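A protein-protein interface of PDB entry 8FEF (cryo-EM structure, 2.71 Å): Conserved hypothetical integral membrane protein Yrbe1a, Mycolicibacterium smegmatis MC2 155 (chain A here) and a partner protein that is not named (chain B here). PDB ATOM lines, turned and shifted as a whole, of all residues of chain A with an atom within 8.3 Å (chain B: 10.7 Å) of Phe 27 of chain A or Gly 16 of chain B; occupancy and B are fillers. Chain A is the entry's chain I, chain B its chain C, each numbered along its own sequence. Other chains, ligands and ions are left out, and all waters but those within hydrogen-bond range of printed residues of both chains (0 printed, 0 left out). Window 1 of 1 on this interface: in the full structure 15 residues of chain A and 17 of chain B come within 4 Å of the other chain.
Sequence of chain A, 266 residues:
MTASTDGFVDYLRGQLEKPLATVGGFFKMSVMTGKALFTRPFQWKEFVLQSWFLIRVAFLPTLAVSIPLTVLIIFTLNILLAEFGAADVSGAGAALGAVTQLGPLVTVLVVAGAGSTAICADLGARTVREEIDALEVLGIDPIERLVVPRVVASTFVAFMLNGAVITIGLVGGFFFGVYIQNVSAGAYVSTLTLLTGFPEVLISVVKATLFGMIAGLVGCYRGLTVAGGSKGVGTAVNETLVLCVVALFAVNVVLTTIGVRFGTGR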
ATOM      1  N   LEU A  20      30.221  -1.947  30.567  1.00  0.00           N
ATOM      2  CA  LEU A  20      29.050  -2.552  29.946  1.00  0.00           C
ATOM      3  C   LEU A  20      27.824  -2.461  30.845  1.00  0.00           C
ATOM      4  O   LEU A  20      26.700  -2.389  30.343  1.00  0.00           O
ATOM      5  CB  LEU A  20      29.347  -4.007  29.591  1.00  0.00           C
ATOM      6  CG  LEU A  20      28.638  -4.585  28.368  1.00  0.00           C
ATOM      7  CD1 LEU A  20      28.723  -3.624  27.196  1.00  0.00           C
ATOM      8  CD2 LEU A  20      29.264  -5.919  28.008  1.00  0.00           C
ATOM      9  N   ALA A  21      28.017  -2.455  32.166  1.00  0.00           N
ATOM     10  CA  ALA A  21      26.889  -2.274  33.076  1.00  0.00           C
ATOM     11  C   ALA A  21      26.260  -0.894  32.910  1.00  0.00           C
ATOM     12  O   ALA A  21      25.033  -0.764  32.826  1.00  0.00           O
ATOM     13  CB  ALA A  21      27.339  -2.493  34.520  1.00  0.00           C
ATOM     14  N   THR A  22      27.088   0.152  32.849  1.00  0.00           N
ATOM     15  CA  THR A  22      26.558   1.495  32.628  1.00  0.00           C
ATOM     16  C   THR A  22      25.947   1.626  31.239  1.00  0.00           C
ATOM     17  O   THR A  22      24.936   2.315  31.060  1.00  0.00           O
ATOM     18  CB  THR A  22      27.658   2.535  32.833  1.00  0.00           C
ATOM     19  OG1 THR A  22      28.775   2.223  31.990  1.00  0.00           O
ATOM     20  CG2 THR A  22      28.113   2.547  34.284  1.00  0.00           C
ATOM     21  N   VAL A  23      26.549   0.967  30.245  1.00  0.00           N
ATOM     22  CA  VAL A  23      25.975   0.947  28.901  1.00  0.00           C
ATOM     23  C   VAL A  23      24.585   0.322  28.922  1.00  0.00           C
ATOM     24  O   VAL A  23      23.639   0.847  28.319  1.00  0.00           O
ATOM     25  CB  VAL A  23      26.924   0.208  27.938  1.00  0.00           C
ATOM     26  CG1 VAL A  23      26.202  -0.199  26.673  1.00  0.00           C
ATOM     27  CG2 VAL A  23      28.123   1.081  27.607  1.00  0.00           C
ATOM     28  N   GLY A  24      24.437  -0.801  29.627  1.00  0.00           N
ATOM     29  CA  GLY A  24      23.139  -1.447  29.719  1.00  0.00           C
ATOM     30  C   GLY A  24      22.123  -0.619  30.479  1.00  0.00           C
ATOM     31  O   GLY A  24      20.942  -0.599  30.127  1.00  0.00           O
ATOM     32  N   GLY A  25      22.564   0.062  31.536  1.00  0.00           N
ATOM     33  CA  GLY A  25      21.671   0.967  32.240  1.00  0.00           C
ATOM     34  C   GLY A  25      21.169   2.084  31.348  1.00  0.00           C
ATOM     35  O   GLY A  25      19.974   2.396  31.338  1.00  0.00           O
ATOM     36  N   PHE A  26      22.071   2.685  30.567  1.00  0.00           N
ATOM     37  CA  PHE A  26      21.671   3.733  29.631  1.00  0.00           C
ATOM     38  C   PHE A  26      20.696   3.203  28.586  1.00  0.00           C
ATOM     39  O   PHE A  26      19.693   3.856  28.276  1.00  0.00           O
ATOM     40  CB  PHE A  26      22.909   4.328  28.958  1.00  0.00           C
ATOM     41  CG  PHE A  26      22.597   5.284  27.840  1.00  0.00           C
ATOM     42  CD1 PHE A  26      22.241   6.592  28.109  1.00  0.00           C
ATOM     43  CD2 PHE A  26      22.682   4.877  26.519  1.00  0.00           C
ATOM     44  CE1 PHE A  26      21.959   7.471  27.084  1.00  0.00           C
ATOM     45  CE2 PHE A  26      22.400   5.753  25.490  1.00  0.00           C
ATOM     46  CZ  PHE A  26      22.039   7.052  25.774  1.00  0.00           C
ATOM     47  N   PHE A  27      20.977   2.021  28.030  1.00  0.00           N
ATOM     48  CA  PHE A  27      20.103   1.463  27.002  1.00  0.00           C
ATOM     49  C   PHE A  27      18.725   1.119  27.556  1.00  0.00           C
ATOM     50  O   PHE A  27      17.708   1.397  26.912  1.00  0.00           O
ATOM     51  CB  PHE A  27      20.760   0.241  26.365  1.00  0.00           C
ATOM     52  CG  PHE A  27      21.803   0.587  25.344  1.00  0.00           C
ATOM     53  CD1 PHE A  27      21.733   1.781  24.646  1.00  0.00           C
ATOM     54  CD2 PHE A  27      22.853  -0.273  25.083  1.00  0.00           C
ATOM     55  CE1 PHE A  27      22.688   2.109  23.704  1.00  0.00           C
ATOM     56  CE2 PHE A  27      23.808   0.047  24.137  1.00  0.00           C
ATOM     57  CZ  PHE A  27      23.726   1.240  23.451  1.00  0.00           C
ATOM     58  N   LYS A  28      18.670   0.519  28.748  1.00  0.00           N
ATOM     59  CA  LYS A  28      17.384   0.199  29.356  1.00  0.00           C
ATOM     60  C   LYS A  28      16.604   1.463  29.686  1.00  0.00           C
ATOM     61  O   LYS A  28      15.381   1.516  29.503  1.00  0.00           O
ATOM     62  CB  LYS A  28      17.597  -0.647  30.611  1.00  0.00           C
ATOM     63  CG  LYS A  28      16.320  -1.002  31.348  1.00  0.00           C
ATOM     64  CD  LYS A  28      16.601  -1.938  32.509  1.00  0.00           C
ATOM     65  CE  LYS A  28      17.698  -1.388  33.401  1.00  0.00           C
ATOM     66  NZ  LYS A  28      17.373  -0.022  33.893  1.00  0.00           N
ATOM     67  N   MET A  29      17.297   2.497  30.172  1.00  0.00           N
ATOM     68  CA  MET A  29      16.639   3.765  30.457  1.00  0.00           C
ATOM     69  C   MET A  29      16.081   4.396  29.186  1.00  0.00           C
ATOM     70  O   MET A  29      14.973   4.943  29.192  1.00  0.00           O
ATOM     71  CB  MET A  29      17.624   4.700  31.152  1.00  0.00           C
ATOM     72  CG  MET A  29      17.050   6.027  31.567  1.00  0.00           C
ATOM     73  SD  MET A  29      17.619   7.351  30.498  1.00  0.00           S
ATOM     74  CE  MET A  29      17.389   8.731  31.598  1.00  0.00           C
ATOM     75  N   SER A  30      16.830   4.326  28.082  1.00  0.00           N
ATOM     76  CA  SER A  30      16.340   4.874  26.819  1.00  0.00           C
ATOM     77  C   SER A  30      15.144   4.085  26.295  1.00  0.00           C
ATOM     78  O   SER A  30      14.203   4.668  25.742  1.00  0.00           O
ATOM     79  CB  SER A  30      17.465   4.899  25.787  1.00  0.00           C
ATOM     80  OG  SER A  30      17.995   3.603  25.579  1.00  0.00           O
ATOM     81  N   VAL A  31      15.170   2.759  26.444  1.00  0.00           N
ATOM     82  CA  VAL A  31      14.033   1.939  26.026  1.00  0.00           C
ATOM     83  C   VAL A  31      12.794   2.294  26.840  1.00  0.00           C
ATOM     84  O   VAL A  31      11.689   2.425  26.295  1.00  0.00           O
ATOM     85  CB  VAL A  31      14.380   0.443  26.138  1.00  0.00           C
ATOM     86  CG1 VAL A  31      13.139  -0.409  25.944  1.00  0.00           C
ATOM     87  CG2 VAL A  31      15.429   0.068  25.108  1.00  0.00           C
ATOM     88  N   MET A  32      12.957   2.461  28.155  1.00  0.00           N
ATOM     89  CA  MET A  32      11.830   2.868  28.991  1.00  0.00           C
ATOM     90  C   MET A  32      11.341   4.263  28.625  1.00  0.00           C
ATOM     91  O   MET A  32      10.137   4.538  28.675  1.00  0.00           O
ATOM     92  CB  MET A  32      12.219   2.797  30.467  1.00  0.00           C
ATOM     93  CG  MET A  32      12.271   1.382  31.020  1.00  0.00           C
ATOM     94  SD  MET A  32      12.493   1.320  32.808  1.00  0.00           S
ATOM     95  CE  MET A  32      14.182   1.887  32.964  1.00  0.00           C
ATOM     96  N   THR A  33      12.259   5.160  28.256  1.00  0.00           N
ATOM     97  CA  THR A  33      11.865   6.496  27.816  1.00  0.00           C
ATOM     98  C   THR A  33      11.027   6.435  26.544  1.00  0.00           C
ATOM     99  O   THR A  33      10.010   7.126  26.426  1.00  0.00           O
ATOM    100  CB  THR A  33      13.108   7.358  27.597  1.00  0.00           C
ATOM    101  OG1 THR A  33      13.850   7.446  28.818  1.00  0.00           O
ATOM    102  CG2 THR A  33      12.725   8.757  27.141  1.00  0.00           C
ATOM    103  N   GLY A  34      11.440   5.608  25.582  1.00  0.00           N
ATOM    104  CA  GLY A  34      10.651   5.445  24.371  1.00  0.00           C
ATOM    105  C   GLY A  34       9.285   4.842  24.644  1.00  0.00           C
ATOM    106  O   GLY A  34       8.277   5.267  24.066  1.00  0.00           O
ATOM    107  N   LEU A 217      19.419  12.043  26.005  1.00  0.00           N
ATOM    108  CA  LEU A 217      19.435  10.754  26.692  1.00  0.00           C
ATOM    109  C   LEU A 217      20.646  10.626  27.610  1.00  0.00           C
ATOM    110  O   LEU A 217      20.518  10.202  28.765  1.00  0.00           O
ATOM    111  CB  LEU A 217      19.414   9.616  25.672  1.00  0.00           C
ATOM    112  CG  LEU A 217      18.093   9.337  24.958  1.00  0.00           C
ATOM    113  CD1 LEU A 217      18.286   8.276  23.891  1.00  0.00           C
ATOM    114  CD2 LEU A 217      17.043   8.901  25.958  1.00  0.00           C
ATOM    115  N   TYR A 221      20.487  10.355  31.681  1.00  0.00           N
ATOM    116  CA  TYR A 221      20.986   9.149  32.334  1.00  0.00           C
ATOM    117  C   TYR A 221      22.094   9.466  33.327  1.00  0.00           C
ATOM    118  O   TYR A 221      22.142   8.884  34.415  1.00  0.00           O
ATOM    119  CB  TYR A 221      21.481   8.144  31.299  1.00  0.00           C
ATOM    120  CG  TYR A 221      22.077   6.906  31.926  1.00  0.00           C
ATOM    121  CD1 TYR A 221      21.283   6.019  32.638  1.00  0.00           C
ATOM    122  CD2 TYR A 221      23.431   6.630  31.817  1.00  0.00           C
ATOM    123  CE1 TYR A 221      21.819   4.890  33.219  1.00  0.00           C
ATOM    124  CE2 TYR A 221      23.977   5.502  32.394  1.00  0.00           C
ATOM    125  CZ  TYR A 221      23.165   4.636  33.094  1.00  0.00           C
ATOM    126  OH  TYR A 221      23.703   3.510  33.672  1.00  0.00           O
ATOM    127  N   THR B   3      15.316   0.236  39.253  1.00  0.00           N
ATOM    128  CA  THR B   3      15.368  -0.365  37.923  1.00  0.00           C
ATOM    129  C   THR B   3      16.698  -0.089  37.234  1.00  0.00           C
ATOM    130  O   THR B   3      17.269  -0.984  36.599  1.00  0.00           O
ATOM    131  CB  THR B   3      14.210   0.151  37.069  1.00  0.00           C
ATOM    132  OG1 THR B   3      14.233   1.584  37.043  1.00  0.00           O
ATOM    133  CG2 THR B   3      12.878  -0.319  37.637  1.00  0.00           C
ATOM    134  N   LEU B   4      17.203   1.144  37.339  1.00  0.00           N
ATOM    135  CA  LEU B   4      18.470   1.485  36.699  1.00  0.00           C
ATOM    136  C   LEU B   4      19.627   0.691  37.292  1.00  0.00           C
ATOM    137  O   LEU B   4      20.495   0.202  36.558  1.00  0.00           O
ATOM    138  CB  LEU B   4      18.735   2.986  36.818  1.00  0.00           C
ATOM    139  CG  LEU B   4      17.760   3.909  36.084  1.00  0.00           C
ATOM    140  CD1 LEU B   4      18.246   5.349  36.136  1.00  0.00           C
ATOM    141  CD2 LEU B   4      17.570   3.456  34.648  1.00  0.00           C
ATOM    142  N   ASP B   8      20.488  -6.472  35.939  1.00  0.00           N
ATOM    143  CA  ASP B   8      20.184  -6.911  34.582  1.00  0.00           C
ATOM    144  C   ASP B   8      20.914  -6.070  33.541  1.00  0.00           C
ATOM    145  O   ASP B   8      20.555  -6.105  32.360  1.00  0.00           O
ATOM    146  CB  ASP B   8      18.675  -6.875  34.324  1.00  0.00           C
ATOM    147  CG  ASP B   8      18.125  -5.461  34.277  1.00  0.00           C
ATOM    148  OD1 ASP B   8      18.630  -4.598  35.024  1.00  0.00           O
ATOM    149  OD2 ASP B   8      17.187  -5.214  33.489  1.00  0.00           O
ATOM    150  N   ARG B   9      21.933  -5.315  33.958  1.00  0.00           N
ATOM    151  CA  ARG B   9      22.565  -4.357  33.059  1.00  0.00           C
ATOM    152  C   ARG B   9      23.446  -5.035  32.016  1.00  0.00           C
ATOM    153  O   ARG B   9      23.638  -4.487  30.927  1.00  0.00           O
ATOM    154  CB  ARG B   9      23.383  -3.353  33.869  1.00  0.00           C
ATOM    155  CG  ARG B   9      22.555  -2.334  34.638  1.00  0.00           C
ATOM    156  CD  ARG B   9      23.453  -1.450  35.491  1.00  0.00           C
ATOM    157  NE  ARG B   9      22.856  -0.149  35.769  1.00  0.00           N
ATOM    158  CZ  ARG B   9      23.494   0.855  36.354  1.00  0.00           C
ATOM    159  NH1 ARG B   9      24.754   0.742  36.741  1.00  0.00           N
ATOM    160  NH2 ARG B   9      22.853   2.004  36.551  1.00  0.00           N
ATOM    161  N   PHE B  10      23.996  -6.212  32.325  1.00  0.00           N
ATOM    162  CA  PHE B  10      24.898  -6.880  31.388  1.00  0.00           C
ATOM    163  C   PHE B  10      24.155  -7.342  30.139  1.00  0.00           C
ATOM    164  O   PHE B  10      24.586  -7.074  29.007  1.00  0.00           O
ATOM    165  CB  PHE B  10      25.586  -8.056  32.080  1.00  0.00           C
ATOM    166  CG  PHE B  10      26.582  -8.775  31.214  1.00  0.00           C
ATOM    167  CD1 PHE B  10      27.852  -8.257  31.025  1.00  0.00           C
ATOM    168  CD2 PHE B  10      26.252  -9.971  30.600  1.00  0.00           C
ATOM    169  CE1 PHE B  10      28.773  -8.914  30.232  1.00  0.00           C
ATOM    170  CE2 PHE B  10      27.169 -10.634  29.806  1.00  0.00           C
ATOM    171  CZ  PHE B  10      28.432 -10.105  29.623  1.00  0.00           C
ATOM    172  N   ARG B  11      23.038  -8.049  30.327  1.00  0.00           N
ATOM    173  CA  ARG B  11      22.248  -8.520  29.194  1.00  0.00           C
ATOM    174  C   ARG B  11      21.659  -7.353  28.415  1.00  0.00           C
ATOM    175  O   ARG B  11      21.607  -7.385  27.178  1.00  0.00           O
ATOM    176  CB  ARG B  11      21.146  -9.458  29.688  1.00  0.00           C
ATOM    177  CG  ARG B  11      20.126  -9.853  28.635  1.00  0.00           C
ATOM    178  CD  ARG B  11      19.262 -11.003  29.122  1.00  0.00           C
ATOM    179  NE  ARG B  11      18.762 -10.771  30.472  1.00  0.00           N
ATOM    180  CZ  ARG B  11      18.046 -11.646  31.166  1.00  0.00           C
ATOM    181  NH1 ARG B  11      17.722 -12.827  30.665  1.00  0.00           N
ATOM    182  NH2 ARG B  11      17.647 -11.329  32.394  1.00  0.00           N
ATOM    183  N   LYS B  12      21.209  -6.316  29.126  1.00  0.00           N
ATOM    184  CA  LYS B  12      20.700  -5.122  28.462  1.00  0.00           C
ATOM    185  C   LYS B  12      21.779  -4.470  27.608  1.00  0.00           C
ATOM    186  O   LYS B  12      21.510  -4.037  26.483  1.00  0.00           O
ATOM    187  CB  LYS B  12      20.164  -4.134  29.499  1.00  0.00           C
ATOM    188  CG  LYS B  12      18.659  -3.940  29.452  1.00  0.00           C
ATOM    189  CD  LYS B  12      17.923  -5.259  29.612  1.00  0.00           C
ATOM    190  CE  LYS B  12      16.419  -5.067  29.512  1.00  0.00           C
ATOM    191  NZ  LYS B  12      15.687  -6.361  29.596  1.00  0.00           N
ATOM    192  N   GLY B  13      23.009  -4.402  28.122  1.00  0.00           N
ATOM    193  CA  GLY B  13      24.097  -3.828  27.348  1.00  0.00           C
ATOM    194  C   GLY B  13      24.437  -4.648  26.122  1.00  0.00           C
ATOM    195  O   GLY B  13      24.663  -4.097  25.041  1.00  0.00           O
ATOM    196  N   LEU B  14      24.480  -5.976  26.272  1.00  0.00           N
ATOM    197  CA  LEU B  14      24.720  -6.846  25.123  1.00  0.00           C
ATOM    198  C   LEU B  14      23.659  -6.638  24.049  1.00  0.00           C
ATOM    199  O   LEU B  14      23.981  -6.414  22.875  1.00  0.00           O
ATOM    200  CB  LEU B  14      24.751  -8.310  25.562  1.00  0.00           C
ATOM    201  CG  LEU B  14      26.125  -8.961  25.726  1.00  0.00           C
ATOM    202  CD1 LEU B  14      26.839  -8.392  26.932  1.00  0.00           C
ATOM    203  CD2 LEU B  14      25.993 -10.471  25.840  1.00  0.00           C
ATOM    204  N   MET B  15      22.384  -6.690  24.444  1.00  0.00           N
ATOM    205  CA  MET B  15      21.302  -6.542  23.477  1.00  0.00           C
ATOM    206  C   MET B  15      21.334  -5.168  22.821  1.00  0.00           C
ATOM    207  O   MET B  15      21.169  -5.053  21.601  1.00  0.00           O
ATOM    208  CB  MET B  15      19.955  -6.782  24.160  1.00  0.00           C
ATOM    209  CG  MET B  15      18.771  -6.806  23.207  1.00  0.00           C
ATOM    210  SD  MET B  15      17.238  -7.305  24.014  1.00  0.00           S
ATOM    211  CE  MET B  15      17.092  -6.040  25.272  1.00  0.00           C
ATOM    212  N   GLY B  16      21.570  -4.118  23.609  1.00  0.00           N
ATOM    213  CA  GLY B  16      21.585  -2.776  23.053  1.00  0.00           C
ATOM    214  C   GLY B  16      22.735  -2.537  22.095  1.00  0.00           C
ATOM    215  O   GLY B  16      22.552  -1.920  21.042  1.00  0.00           O
ATOM    216  N   VAL B  17      23.937  -3.011  22.440  1.00  0.00           N
ATOM    217  CA  VAL B  17      25.071  -2.812  21.543  1.00  0.00           C
ATOM    218  C   VAL B  17      24.896  -3.637  20.271  1.00  0.00           C
ATOM    219  O   VAL B  17      25.259  -3.186  19.175  1.00  0.00           O
ATOM    220  CB  VAL B  17      26.405  -3.105  22.263  1.00  0.00           C
ATOM    221  CG1 VAL B  17      26.613  -4.593  22.520  1.00  0.00           C
ATOM    222  CG2 VAL B  17      27.571  -2.524  21.474  1.00  0.00           C
ATOM    223  N   ILE B  18      24.311  -4.836  20.380  1.00  0.00           N
ATOM    224  CA  ILE B  18      24.026  -5.625  19.184  1.00  0.00           C
ATOM    225  C   ILE B  18      23.020  -4.901  18.297  1.00  0.00           C
ATOM    226  O   ILE B  18      23.184  -4.839  17.073  1.00  0.00           O
ATOM    227  CB  ILE B  18      23.542  -7.036  19.570  1.00  0.00           C
ATOM    228  CG1 ILE B  18      24.702  -7.856  20.141  1.00  0.00           C
ATOM    229  CG2 ILE B  18      22.927  -7.747  18.373  1.00  0.00           C
ATOM    230  CD1 ILE B  18      24.312  -9.254  20.564  1.00  0.00           C
ATOM    231  N   VAL B  19      21.975  -4.327  18.902  1.00  0.00           N
ATOM    232  CA  VAL B  19      20.965  -3.608  18.128  1.00  0.00           C
ATOM    233  C   VAL B  19      21.572  -2.386  17.447  1.00  0.00           C
ATOM    234  O   VAL B  19      21.285  -2.108  16.279  1.00  0.00           O
ATOM    235  CB  VAL B  19      19.771  -3.232  19.027  1.00  0.00           C
ATOM    236  CG1 VAL B  19      18.878  -2.210  18.342  1.00  0.00           C
ATOM    237  CG2 VAL B  19      18.964  -4.471  19.367  1.00  0.00           C
ATOM    238  N   VAL B  20      22.419  -1.640  18.162  1.00  0.00           N
ATOM    239  CA  VAL B  20      23.036  -0.449  17.577  1.00  0.00           C
ATOM    240  C   VAL B  20      23.957  -0.829  16.421  1.00  0.00           C
ATOM    241  O   VAL B  20      23.954  -0.180  15.366  1.00  0.00           O
ATOM    242  CB  VAL B  20      23.778   0.357  18.659  1.00  0.00           C
ATOM    243  CG1 VAL B  20      24.621   1.454  18.028  1.00  0.00           C
ATOM    244  CG2 VAL B  20      22.784   0.965  19.632  1.00  0.00           C
ATOM    245  N   ALA B  21      24.757  -1.888  16.598  1.00  0.00           N
ATOM    246  CA  ALA B  21      25.627  -2.339  15.516  1.00  0.00           C
ATOM    247  C   ALA B  21      24.818  -2.794  14.307  1.00  0.00           C
ATOM    248  O   ALA B  21      25.174  -2.489  13.162  1.00  0.00           O
ATOM    249  CB  ALA B  21      26.536  -3.465  16.009  1.00  0.00           C
ATOM    250  N   LEU B  22      23.720  -3.520  14.543  1.00  0.00           N
ATOM    251  CA  LEU B  22      22.866  -3.956  13.443  1.00  0.00           C
ATOM    252  C   LEU B  22      22.236  -2.770  12.725  1.00  0.00           C
ATOM    253  O   LEU B  22      22.132  -2.769  11.494  1.00  0.00           O
ATOM    254  CB  LEU B  22      21.787  -4.909  13.956  1.00  0.00           C
ATOM    255  CG  LEU B  22      22.248  -6.315  14.345  1.00  0.00           C
ATOM    256  CD1 LEU B  22      21.066  -7.167  14.780  1.00  0.00           C
ATOM    257  CD2 LEU B  22      22.996  -6.973  13.198  1.00  0.00           C
ATOM    258  N   ILE B  23      21.793  -1.761  13.477  1.00  0.00           N
ATOM    259  CA  ILE B  23      21.203  -0.570  12.867  1.00  0.00           C
ATOM    260  C   ILE B  23      22.227   0.146  11.995  1.00  0.00           C
ATOM    261  O   ILE B  23      21.928   0.550  10.867  1.00  0.00           O
ATOM    262  CB  ILE B  23      20.628   0.362  13.949  1.00  0.00           C
ATOM    263  CG1 ILE B  23      19.362  -0.242  14.560  1.00  0.00           C
ATOM    264  CG2 ILE B  23      20.336   1.743  13.381  1.00  0.00           C
ATOM    265  CD1 ILE B  23      18.731   0.622  15.629  1.00  0.00           C
ATOM    266  N   ILE B  24      23.447   0.322  12.509  1.00  0.00           N
ATOM    267  CA  ILE B  24      24.494   0.990  11.735  1.00  0.00           C
ATOM    268  C   ILE B  24      24.832   0.200  10.474  1.00  0.00           C
ATOM    269  O   ILE B  24      24.951   0.768   9.377  1.00  0.00           O
ATOM    270  CB  ILE B  24      25.738   1.223  12.613  1.00  0.00           C
ATOM    271  CG1 ILE B  24      25.423   2.225  13.726  1.00  0.00           C
ATOM    272  CG2 ILE B  24      26.910   1.707  11.773  1.00  0.00           C
ATOM    273  CD1 ILE B  24      26.600   2.542  14.621  1.00  0.00           C
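The side-chain amino group (NZ) of Lys 28 of chain A is in hydrogen-bond range of the backbone carbonyl oxygen (O) of Thr 3 of chain B, 2.9 Å away. The guanidinium group (NH2) of Arg 9 of chain B lies within hydrogen-bond range of the side-chain hydroxyl (OH) of Tyr 221 of chain A, 3.4 Å away.
The guanidinium group of Arg 9 of chain B is in hydrogen-bond range of the backbone carbonyl oxygen of Leu 4 of chain B, at 2.5 Å. The backbone carbonyl oxygen (O) of Thr 22 of chain A lies within hydrogen-bond range of the side-chain hydroxyl (OH) of Tyr 221 of chain A (3.1 Å). O of Phe 27 of chain A lies within hydrogen-bond range of OG of Ser 30 of chain A, 2.6 Å away. O of Met 29 of chain A sits at hydrogen-bond distance from OG1 of Thr 33 of chain A.
Of chain A, only Phe 27 comes within 4 Å of Gly 16 of chain B. Gly 24 of chain A touches just these residues of chain B: Arg 9, Lys 12 and Gly 13. Printed residues of chain B within 4 Å of Gly 25 of chain A: Arg 9. No residue of chain B comes within 4 Å of Phe 26 of chain A. No residue of chain B comes within 4 Å of Ser 30 of chain A. Of the printed residues of chain A, Thr 3 of chain B touches Lys 28. Of the printed residues of chain B, Leu 20 of chain A touches Arg 9, Phe 10 and Leu 14. Leu 217 of chain A touches none of the printed residues of chain B.
Arg 9 of chain B touches Leu 20 of chain A (O to O, 3.8 Å). Gly 24 of chain A touches Arg 9 of chain B. Lys 12 of chain B touches Gly 24 of chain A. Gly 25 of chain A touches Arg 9 of chain B. Phe 27 of chain A touches Gly 16 of chain B. Phe 27 of chain A touches Val 17 of chain B. CZ of Phe 27 of chain A touches CG2 of Val 20 of chain B, 3.9 Å away. Lys 28 of chain A touches Leu 4 of chain B. Lys 28 of chain A touches Asp 8 of chain B (CD to OD2, 3.5 Å). Leu 4 of chain B touches Met 29 of chain A (CD2 to CB, 3.7 Å).
Hydrophobic or aromatic side chains of chain B within 4 Å of the printed part of chain A: Leu 4, Phe 10, Leu 14 and Val 20. Of the 17 printed residues of chain A, 8 touch a printed residue of chain B. Among the printed residues, no Asp or Glu carboxylate lies within 4 Å of a Lys or Arg side-chain nitrogen of the other chain.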
